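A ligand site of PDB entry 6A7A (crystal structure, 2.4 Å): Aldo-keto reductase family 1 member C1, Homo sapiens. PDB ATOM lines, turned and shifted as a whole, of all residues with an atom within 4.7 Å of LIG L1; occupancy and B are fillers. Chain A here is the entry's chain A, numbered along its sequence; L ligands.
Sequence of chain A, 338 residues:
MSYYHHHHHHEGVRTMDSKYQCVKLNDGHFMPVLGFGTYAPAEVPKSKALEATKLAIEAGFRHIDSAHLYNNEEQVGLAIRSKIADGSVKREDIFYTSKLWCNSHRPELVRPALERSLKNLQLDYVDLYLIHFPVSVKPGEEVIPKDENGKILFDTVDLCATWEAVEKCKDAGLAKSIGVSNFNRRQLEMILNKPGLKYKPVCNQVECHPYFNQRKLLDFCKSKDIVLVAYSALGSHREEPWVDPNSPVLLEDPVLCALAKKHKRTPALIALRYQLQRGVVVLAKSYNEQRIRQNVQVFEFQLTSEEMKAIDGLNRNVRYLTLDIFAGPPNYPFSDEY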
ATOM      1  N   TYR A  39     -23.064 -33.674  -5.015  1.00  0.00           N
ATOM      2  CA  TYR A  39     -24.074 -32.917  -4.274  1.00  0.00           C
ATOM      3  C   TYR A  39     -25.450 -33.144  -4.855  1.00  0.00           C
ATOM      4  O   TYR A  39     -25.636 -33.158  -6.079  1.00  0.00           O
ATOM      5  CB  TYR A  39     -23.801 -31.412  -4.245  1.00  0.00           C
ATOM      6  CG  TYR A  39     -24.945 -30.691  -3.605  1.00  0.00           C
ATOM      7  CD1 TYR A  39     -25.107 -30.711  -2.231  1.00  0.00           C
ATOM      8  CD2 TYR A  39     -25.910 -30.060  -4.374  1.00  0.00           C
ATOM      9  CE1 TYR A  39     -26.186 -30.077  -1.619  1.00  0.00           C
ATOM     10  CE2 TYR A  39     -26.990 -29.423  -3.779  1.00  0.00           C
ATOM     11  CZ  TYR A  39     -27.130 -29.435  -2.406  1.00  0.00           C
ATOM     12  OH  TYR A  39     -28.199 -28.807  -1.820  1.00  0.00           O
ATOM     13  N   LEU A  69     -19.938 -30.335   3.824  1.00  0.00           N
ATOM     14  CA  LEU A  69     -21.252 -29.720   3.676  1.00  0.00           C
ATOM     15  C   LEU A  69     -22.312 -30.640   3.050  1.00  0.00           C
ATOM     16  O   LEU A  69     -23.490 -30.533   3.404  1.00  0.00           O
ATOM     17  CB  LEU A  69     -21.171 -28.454   2.822  1.00  0.00           C
ATOM     18  CG  LEU A  69     -22.509 -27.730   2.612  1.00  0.00           C
ATOM     19  CD1 LEU A  69     -23.050 -27.131   3.926  1.00  0.00           C
ATOM     20  CD2 LEU A  69     -22.411 -26.664   1.530  1.00  0.00           C
ATOM     21  N   TYR A  70     -21.919 -31.535   2.148  1.00  0.00           N
ATOM     22  CA  TYR A  70     -22.916 -32.290   1.381  1.00  0.00           C
ATOM     23  C   TYR A  70     -23.546 -33.424   2.196  1.00  0.00           C
ATOM     24  O   TYR A  70     -24.557 -33.987   1.775  1.00  0.00           O
ATOM     25  CB  TYR A  70     -22.314 -32.862   0.091  1.00  0.00           C
ATOM     26  CG  TYR A  70     -21.628 -31.856  -0.808  1.00  0.00           C
ATOM     27  CD1 TYR A  70     -21.883 -30.500  -0.684  1.00  0.00           C
ATOM     28  CD2 TYR A  70     -20.716 -32.275  -1.774  1.00  0.00           C
ATOM     29  CE1 TYR A  70     -21.250 -29.573  -1.495  1.00  0.00           C
ATOM     30  CE2 TYR A  70     -20.082 -31.367  -2.596  1.00  0.00           C
ATOM     31  CZ  TYR A  70     -20.348 -30.013  -2.453  1.00  0.00           C
ATOM     32  OH  TYR A  70     -19.710 -29.103  -3.251  1.00  0.00           O
ATOM     33  N   TRP A 101     -15.587 -27.016   5.585  1.00  0.00           N
ATOM     34  CA  TRP A 101     -16.696 -26.072   5.611  1.00  0.00           C
ATOM     35  C   TRP A 101     -16.397 -24.883   6.523  1.00  0.00           C
ATOM     36  O   TRP A 101     -15.523 -24.944   7.396  1.00  0.00           O
ATOM     37  CB  TRP A 101     -18.011 -26.753   6.038  1.00  0.00           C
ATOM     38  CG  TRP A 101     -19.146 -25.783   5.912  1.00  0.00           C
ATOM     39  CD1 TRP A 101     -19.956 -25.319   6.913  1.00  0.00           C
ATOM     40  CD2 TRP A 101     -19.525 -25.064   4.722  1.00  0.00           C
ATOM     41  NE1 TRP A 101     -20.839 -24.389   6.403  1.00  0.00           N
ATOM     42  CE2 TRP A 101     -20.594 -24.219   5.073  1.00  0.00           C
ATOM     43  CE3 TRP A 101     -19.077 -25.085   3.396  1.00  0.00           C
ATOM     44  CZ2 TRP A 101     -21.231 -23.398   4.146  1.00  0.00           C
ATOM     45  CZ3 TRP A 101     -19.714 -24.263   2.469  1.00  0.00           C
ATOM     46  CH2 TRP A 101     -20.766 -23.430   2.850  1.00  0.00           C
ATOM     47  N   HIS A 132     -13.660 -24.561   1.357  1.00  0.00           N
ATOM     48  CA  HIS A 132     -14.881 -24.614   0.568  1.00  0.00           C
ATOM     49  C   HIS A 132     -15.381 -23.236   0.134  1.00  0.00           C
ATOM     50  O   HIS A 132     -15.804 -23.047  -1.010  1.00  0.00           O
ATOM     51  CB  HIS A 132     -15.965 -25.347   1.362  1.00  0.00           C
ATOM     52  CG  HIS A 132     -17.084 -25.899   0.526  1.00  0.00           C
ATOM     53  ND1 HIS A 132     -17.755 -27.058   0.850  1.00  0.00           N
ATOM     54  CD2 HIS A 132     -17.666 -25.425  -0.610  1.00  0.00           C
ATOM     55  CE1 HIS A 132     -18.688 -27.287  -0.061  1.00  0.00           C
ATOM     56  NE2 HIS A 132     -18.659 -26.318  -0.950  1.00  0.00           N
ATOM     57  N   PHE A 133     -15.345 -22.269   1.058  1.00  0.00           N
ATOM     58  CA  PHE A 133     -15.894 -20.930   0.829  1.00  0.00           C
ATOM     59  C   PHE A 133     -15.230 -19.957   1.793  1.00  0.00           C
ATOM     60  O   PHE A 133     -15.025 -20.293   2.950  1.00  0.00           O
ATOM     61  CB  PHE A 133     -17.418 -20.953   1.018  1.00  0.00           C
ATOM     62  CG  PHE A 133     -18.120 -19.718   0.519  1.00  0.00           C
ATOM     63  CD1 PHE A 133     -18.486 -19.596  -0.820  1.00  0.00           C
ATOM     64  CD2 PHE A 133     -18.408 -18.671   1.373  1.00  0.00           C
ATOM     65  CE1 PHE A 133     -19.130 -18.467  -1.285  1.00  0.00           C
ATOM     66  CE2 PHE A 133     -19.050 -17.536   0.915  1.00  0.00           C
ATOM     67  CZ  PHE A 133     -19.413 -17.437  -0.417  1.00  0.00           C
ATOM     68  N   ILE A 144     -24.988 -23.791   8.788  1.00  0.00           N
ATOM     69  CA  ILE A 144     -25.448 -22.415   8.605  1.00  0.00           C
ATOM     70  C   ILE A 144     -26.072 -21.870   9.885  1.00  0.00           C
ATOM     71  O   ILE A 144     -27.299 -21.750   9.967  1.00  0.00           O
ATOM     72  CB  ILE A 144     -26.456 -22.301   7.468  1.00  0.00           C
ATOM     73  CG1 ILE A 144     -25.931 -22.990   6.212  1.00  0.00           C
ATOM     74  CG2 ILE A 144     -26.708 -20.839   7.151  1.00  0.00           C
ATOM     75  CD1 ILE A 144     -26.871 -22.864   5.028  1.00  0.00           C
ATOM     76  N   ASN A 182     -14.222 -20.961  -4.636  1.00  0.00           N
ATOM     77  CA  ASN A 182     -14.934 -19.678  -4.537  1.00  0.00           C
ATOM     78  C   ASN A 182     -14.065 -18.511  -4.052  1.00  0.00           C
ATOM     79  O   ASN A 182     -14.584 -17.599  -3.413  1.00  0.00           O
ATOM     80  CB  ASN A 182     -16.138 -19.800  -3.596  1.00  0.00           C
ATOM     81  CG  ASN A 182     -17.099 -20.899  -4.013  1.00  0.00           C
ATOM     82  OD1 ASN A 182     -17.217 -21.922  -3.336  1.00  0.00           O
ATOM     83  ND2 ASN A 182     -17.786 -20.699  -5.131  1.00  0.00           N
ATOM     84  N   HIS A 237     -27.677 -27.292 -10.467  1.00  0.00           N
ATOM     85  CA  HIS A 237     -28.838 -28.032  -9.958  1.00  0.00           C
ATOM     86  C   HIS A 237     -30.144 -27.236 -10.064  1.00  0.00           C
ATOM     87  O   HIS A 237     -31.224 -27.818 -10.070  1.00  0.00           O
ATOM     88  CB  HIS A 237     -28.614 -28.408  -8.496  1.00  0.00           C
ATOM     89  CG  HIS A 237     -27.933 -27.319  -7.710  1.00  0.00           C
ATOM     90  ND1 HIS A 237     -28.443 -26.040  -7.623  1.00  0.00           N
ATOM     91  CD2 HIS A 237     -26.769 -27.317  -7.022  1.00  0.00           C
ATOM     92  CE1 HIS A 237     -27.623 -25.298  -6.894  1.00  0.00           C
ATOM     93  NE2 HIS A 237     -26.607 -26.052  -6.518  1.00  0.00           N
ATOM     94  N   GLU A 239     -31.575 -25.662  -7.858  1.00  0.00           N
ATOM     95  CA  GLU A 239     -32.373 -25.900  -6.650  1.00  0.00           C
ATOM     96  C   GLU A 239     -32.983 -24.616  -6.103  1.00  0.00           C
ATOM     97  O   GLU A 239     -32.293 -23.612  -5.923  1.00  0.00           O
ATOM     98  CB  GLU A 239     -31.513 -26.571  -5.574  1.00  0.00           C
ATOM     99  CG  GLU A 239     -32.180 -26.718  -4.215  1.00  0.00           C
ATOM    100  CD  GLU A 239     -31.357 -27.536  -3.231  1.00  0.00           C
ATOM    101  OE1 GLU A 239     -31.910 -27.973  -2.192  1.00  0.00           O
ATOM    102  OE2 GLU A 239     -30.159 -27.763  -3.484  1.00  0.00           O
ATOM    103  N   TRP A 242     -32.402 -21.444  -3.902  1.00  0.00           N
ATOM    104  CA  TRP A 242     -31.030 -21.006  -4.214  1.00  0.00           C
ATOM    105  C   TRP A 242     -30.856 -20.418  -5.616  1.00  0.00           C
ATOM    106  O   TRP A 242     -29.923 -19.646  -5.853  1.00  0.00           O
ATOM    107  CB  TRP A 242     -30.062 -22.187  -4.036  1.00  0.00           C
ATOM    108  CG  TRP A 242     -30.105 -22.816  -2.671  1.00  0.00           C
ATOM    109  CD1 TRP A 242     -30.726 -23.994  -2.332  1.00  0.00           C
ATOM    110  CD2 TRP A 242     -29.514 -22.312  -1.470  1.00  0.00           C
ATOM    111  NE1 TRP A 242     -30.541 -24.248  -0.993  1.00  0.00           N
ATOM    112  CE2 TRP A 242     -29.809 -23.235  -0.434  1.00  0.00           C
ATOM    113  CE3 TRP A 242     -28.766 -21.165  -1.162  1.00  0.00           C
ATOM    114  CZ2 TRP A 242     -29.385 -23.048   0.871  1.00  0.00           C
ATOM    115  CZ3 TRP A 242     -28.350 -20.987   0.142  1.00  0.00           C
ATOM    116  CH2 TRP A 242     -28.653 -21.919   1.148  1.00  0.00           C
ATOM    117  N   VAL A 243     -31.745 -20.776  -6.539  1.00  0.00           N
ATOM    118  CA  VAL A 243     -31.545 -20.417  -7.938  1.00  0.00           C
ATOM    119  C   VAL A 243     -32.858 -20.017  -8.616  1.00  0.00           C
ATOM    120  O   VAL A 243     -33.862 -20.732  -8.530  1.00  0.00           O
ATOM    121  CB  VAL A 243     -30.884 -21.579  -8.737  1.00  0.00           C
ATOM    122  CG1 VAL A 243     -30.616 -21.164 -10.154  1.00  0.00           C
ATOM    123  CG2 VAL A 243     -29.582 -22.026  -8.069  1.00  0.00           C
ATOM    124  N   LEU A 321     -25.101 -19.385  -8.753  1.00  0.00           N
ATOM    125  CA  LEU A 321     -24.854 -19.525  -7.315  1.00  0.00           C
ATOM    126  C   LEU A 321     -24.198 -18.263  -6.772  1.00  0.00           C
ATOM    127  O   LEU A 321     -22.997 -18.068  -6.919  1.00  0.00           O
ATOM    128  CB  LEU A 321     -23.989 -20.749  -7.035  1.00  0.00           C
ATOM    129  CG  LEU A 321     -23.748 -21.207  -5.588  1.00  0.00           C
ATOM    130  CD1 LEU A 321     -22.980 -22.520  -5.569  1.00  0.00           C
ATOM    131  CD2 LEU A 321     -23.008 -20.162  -4.742  1.00  0.00           C
ATOM    132  N   LEU A 323     -25.034 -17.096  -3.439  1.00  0.00           N
ATOM    133  CA  LEU A 323     -25.042 -17.215  -1.974  1.00  0.00           C
ATOM    134  C   LEU A 323     -25.223 -15.878  -1.278  1.00  0.00           C
ATOM    135  O   LEU A 323     -24.396 -15.498  -0.450  1.00  0.00           O
ATOM    136  CB  LEU A 323     -23.750 -17.855  -1.477  1.00  0.00           C
ATOM    137  CG  LEU A 323     -23.590 -19.363  -1.627  1.00  0.00           C
ATOM    138  CD1 LEU A 323     -22.216 -19.741  -1.101  1.00  0.00           C
ATOM    139  CD2 LEU A 323     -24.679 -20.098  -0.857  1.00  0.00           C
ATOM    140  N   ILE A 325     -26.910 -14.968   1.056  1.00  0.00           N
ATOM    141  CA  ILE A 325     -27.045 -15.053   2.507  1.00  0.00           C
ATOM    142  C   ILE A 325     -25.675 -14.890   3.175  1.00  0.00           C
ATOM    143  O   ILE A 325     -25.601 -14.531   4.351  1.00  0.00           O
ATOM    144  CB  ILE A 325     -27.673 -16.386   2.958  1.00  0.00           C
ATOM    145  CG1 ILE A 325     -26.772 -17.554   2.568  1.00  0.00           C
ATOM    146  CG2 ILE A 325     -29.069 -16.552   2.358  1.00  0.00           C
ATOM    147  CD1 ILE A 325     -27.240 -18.893   3.107  1.00  0.00           C
ATOM    148  N   PHE A 326     -24.615 -15.144   2.411  1.00  0.00           N
ATOM    149  CA  PHE A 326     -23.243 -14.941   2.903  1.00  0.00           C
ATOM    150  C   PHE A 326     -22.650 -13.580   2.564  1.00  0.00           C
ATOM    151  O   PHE A 326     -21.511 -13.294   2.911  1.00  0.00           O
ATOM    152  CB  PHE A 326     -22.331 -16.053   2.375  1.00  0.00           C
ATOM    153  CG  PHE A 326     -22.377 -17.300   3.200  1.00  0.00           C
ATOM    154  CD1 PHE A 326     -23.511 -17.615   3.914  1.00  0.00           C
ATOM    155  CD2 PHE A 326     -21.273 -18.120   3.299  1.00  0.00           C
ATOM    156  CE1 PHE A 326     -23.563 -18.754   4.700  1.00  0.00           C
ATOM    157  CE2 PHE A 326     -21.315 -19.249   4.086  1.00  0.00           C
ATOM    158  CZ  PHE A 326     -22.461 -19.569   4.782  1.00  0.00           C
HETATM  159  O1  LIG L   1     -27.897 -26.080  -2.005  1.00  0.00           O
HETATM  160  O2  LIG L   1     -20.704 -24.382  -1.526  1.00  0.00           O
HETATM  161  C1  LIG L   1     -25.653 -24.200  -1.802  1.00  0.00           C
HETATM  162  C2  LIG L   1     -26.227 -24.957  -0.623  1.00  0.00           C
HETATM  163  C3  LIG L   1     -24.306 -24.779  -2.222  1.00  0.00           C
HETATM  164  C4  LIG L   1     -27.211 -25.865  -0.842  1.00  0.00           C
HETATM  165  C5  LIG L   1     -26.654 -24.284  -2.958  1.00  0.00           C
HETATM  166  C6  LIG L   1     -23.013 -26.457  -3.333  1.00  0.00           C
HETATM  167  C7  LIG L   1     -24.240 -25.869  -3.085  1.00  0.00           C
HETATM  168  C8  LIG L   1     -27.628 -25.221  -3.030  1.00  0.00           C
HETATM  169  C9  LIG L   1     -25.952 -25.082   0.792  1.00  0.00           C
HETATM  170  N1  LIG L   1     -26.710 -26.022   1.339  1.00  0.00           N
HETATM  171  N2  LIG L   1     -23.003 -27.557  -4.306  1.00  0.00           N
HETATM  172  N3  LIG L   1     -28.525 -25.396  -4.017  1.00  0.00           N
HETATM  173  C10 LIG L   1     -23.132 -24.271  -1.671  1.00  0.00           C
HETATM  174  C11 LIG L   1     -21.909 -24.871  -1.932  1.00  0.00           C
HETATM  175  C12 LIG L   1     -21.838 -26.013  -2.737  1.00  0.00           C
HETATM  176  N4  LIG L   1     -27.508 -26.525   0.347  1.00  0.00           N
HETATM  177  C13 LIG L   1     -20.686 -23.121  -0.858  1.00  0.00           C
HETATM  178  C14 LIG L   1     -25.302 -22.803   1.661  1.00  0.00           C
HETATM  179  C15 LIG L   1     -24.977 -24.282   1.595  1.00  0.00           C
HETATM  180  C16 LIG L   1     -26.534 -23.322  -3.996  1.00  0.00           C
HETATM  181  O3  LIG L   1     -20.679 -26.687  -2.800  1.00  0.00           O
HETATM  182  O4  LIG L   1     -23.894 -27.612  -5.139  1.00  0.00           O
HETATM  183  O5  LIG L   1     -22.087 -28.370  -4.244  1.00  0.00           O
HETATM  184  N5  LIG L   1     -26.458 -22.576  -4.854  1.00  0.00           N
HETATM  185  C17 LIG L   1     -24.206 -21.954   2.338  1.00  0.00           C
HETATM  186  P1  LG2 L   2     -24.293 -29.434 -12.704  1.00  0.00           P
HETATM  187  O1  LG2 L   2     -23.200 -30.427 -12.764  1.00  0.00           O
HETATM  188  O2  LG2 L   2     -24.010 -28.177 -13.523  1.00  0.00           O
HETATM  189  O3  LG2 L   2     -25.711 -30.008 -13.237  1.00  0.00           O
HETATM  190  C1  LG2 L   2     -26.482 -30.826 -12.337  1.00  0.00           C
HETATM  191  C2  LG2 L   2     -27.838 -31.038 -12.952  1.00  0.00           C
HETATM  192  O4  LG2 L   2     -27.691 -31.392 -14.348  1.00  0.00           O
HETATM  193  C3  LG2 L   2     -28.647 -32.157 -12.310  1.00  0.00           C
HETATM  194  O5  LG2 L   2     -29.995 -31.751 -12.123  1.00  0.00           O
HETATM  195  C4  LG2 L   2     -28.573 -33.304 -13.320  1.00  0.00           C
HETATM  196  O6  LG2 L   2     -29.769 -34.105 -13.270  1.00  0.00           O
HETATM  197  C5  LG2 L   2     -28.409 -32.579 -14.646  1.00  0.00           C
HETATM  198  N1  LG2 L   2     -27.650 -33.329 -15.638  1.00  0.00           N
HETATM  199  C6  LG2 L   2     -26.512 -34.068 -15.428  1.00  0.00           C
HETATM  200  N2  LG2 L   2     -26.018 -34.616 -16.509  1.00  0.00           N
HETATM  201  C7  LG2 L   2     -26.888 -34.229 -17.507  1.00  0.00           C
HETATM  202  C8  LG2 L   2     -26.969 -34.548 -18.870  1.00  0.00           C
HETATM  203  N3  LG2 L   2     -26.079 -35.332 -19.502  1.00  0.00           N
HETATM  204  N4  LG2 L   2     -28.013 -34.065 -19.575  1.00  0.00           N
HETATM  205  C9  LG2 L   2     -28.907 -33.297 -18.940  1.00  0.00           C
HETATM  206  N5  LG2 L   2     -28.937 -32.921 -17.660  1.00  0.00           N
HETATM  207  C10 LG2 L   2     -27.902 -33.430 -16.983  1.00  0.00           C
HETATM  208  O7  LG2 L   2     -24.694 -29.038 -11.216  1.00  0.00           O
HETATM  209  P2  LG2 L   2     -24.151 -28.771  -9.732  1.00  0.00           P
HETATM  210  O8  LG2 L   2     -24.640 -29.844  -8.841  1.00  0.00           O
HETATM  211  O9  LG2 L   2     -24.480 -27.373  -9.398  1.00  0.00           O
HETATM  212  O10 LG2 L   2     -22.574 -28.938  -9.894  1.00  0.00           O
HETATM  213  C11 LG2 L   2     -21.969 -30.252  -9.887  1.00  0.00           C
HETATM  214  C12 LG2 L   2     -21.076 -30.443  -8.683  1.00  0.00           C
HETATM  215  O11 LG2 L   2     -20.160 -29.339  -8.504  1.00  0.00           O
HETATM  216  C13 LG2 L   2     -21.743 -30.590  -7.324  1.00  0.00           C
HETATM  217  O12 LG2 L   2     -22.317 -31.880  -7.137  1.00  0.00           O
HETATM  218  C14 LG2 L   2     -20.564 -30.351  -6.396  1.00  0.00           C
HETATM  219  O13 LG2 L   2     -19.686 -31.478  -6.344  1.00  0.00           O
HETATM  220  C15 LG2 L   2     -19.840 -29.217  -7.132  1.00  0.00           C
HETATM  221  N6  LG2 L   2     -20.254 -27.818  -6.645  1.00  0.00           N
HETATM  222  C16 LG2 L   2     -19.369 -27.193  -5.861  1.00  0.00           C
HETATM  223  C17 LG2 L   2     -19.642 -25.927  -5.374  1.00  0.00           C
HETATM  224  C18 LG2 L   2     -18.628 -25.188  -4.529  1.00  0.00           C
HETATM  225  O14 LG2 L   2     -17.475 -25.696  -4.337  1.00  0.00           O
HETATM  226  N7  LG2 L   2     -18.962 -23.990  -4.057  1.00  0.00           N
HETATM  227  C19 LG2 L   2     -20.844 -25.324  -5.717  1.00  0.00           C
HETATM  228  C20 LG2 L   2     -21.735 -25.987  -6.533  1.00  0.00           C
HETATM  229  C21 LG2 L   2     -21.420 -27.246  -7.000  1.00  0.00           C
HETATM  230  P3  LG2 L   2     -29.681 -35.654 -12.902  1.00  0.00           P
HETATM  231  O15 LG2 L   2     -28.980 -35.846 -11.575  1.00  0.00           O
HETATM  232  O16 LG2 L   2     -31.128 -36.128 -12.877  1.00  0.00           O
HETATM  233  O17 LG2 L   2     -28.967 -36.363 -14.094  1.00  0.00           O
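A ring nitrogen (NE2) of His 132 lies within hydrogen-bond range of an oxygen (O3) of LIG L1 (2.8 Å).
The backbone NH (N) of His 237 lies close to an oxygen (O9) of LG2 L2, 3.4 Å away.
N3 of LIG L1 sits close to NE2 of His 237.
A nitrogen (N3) of LIG L1 is in hydrogen-bond range of the side-chain carboxylate (OE2) of Glu 239, at 2.9 Å.
OD1 of Asn 182 is in hydrogen-bond range of N7 of LG2 L2 (2.8 Å).
O12 of LG2 L2 lies within hydrogen-bond range of N of Tyr 39 (2.9 Å).
OH of Tyr 70 sits at hydrogen-bond distance from O3 of LIG L1 (2.6 Å).
The indole nitrogen of Trp 242 lies within hydrogen-bond range of an oxygen (O1) of LIG L1.
The side-chain hydroxyl (OH) of Tyr 39 is in hydrogen-bond range of an oxygen (O1) of LIG L1.
An oxygen (O2) of LIG L1 sits at hydrogen-bond distance from a nitrogen (N7) of LG2 L2, at 3.1 Å.
OD1 of Asn 182 sits close to O of His 132, at 2.9 Å.
The side-chain carboxylate (OE2) of Glu 239 lies within hydrogen-bond range of the side-chain hydroxyl (OH) of Tyr 39.
A ring nitrogen (ND1) of His 237 sits close to the backbone NH (N) of Glu 239, 3.2 Å away.
Residues that only touch LIG L1: Leu 69 (3.5 Å), Trp 101 (3.6 Å), Ile 144 (3.7 Å), Leu 321 (3.1 Å), Leu 323 (3.7 Å) and Phe 326 (3.8 Å).
12 residues have an atom within 4 Å of LIG L1: Tyr 39, Leu 69, Tyr 70, Trp 101, His 132, Ile 144, His 237, Glu 239, Trp 242, Leu 321, Leu 323 and Phe 326.
The nearest printed residue that does not touch LIG L1 is Phe 133 (4.2 Å).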
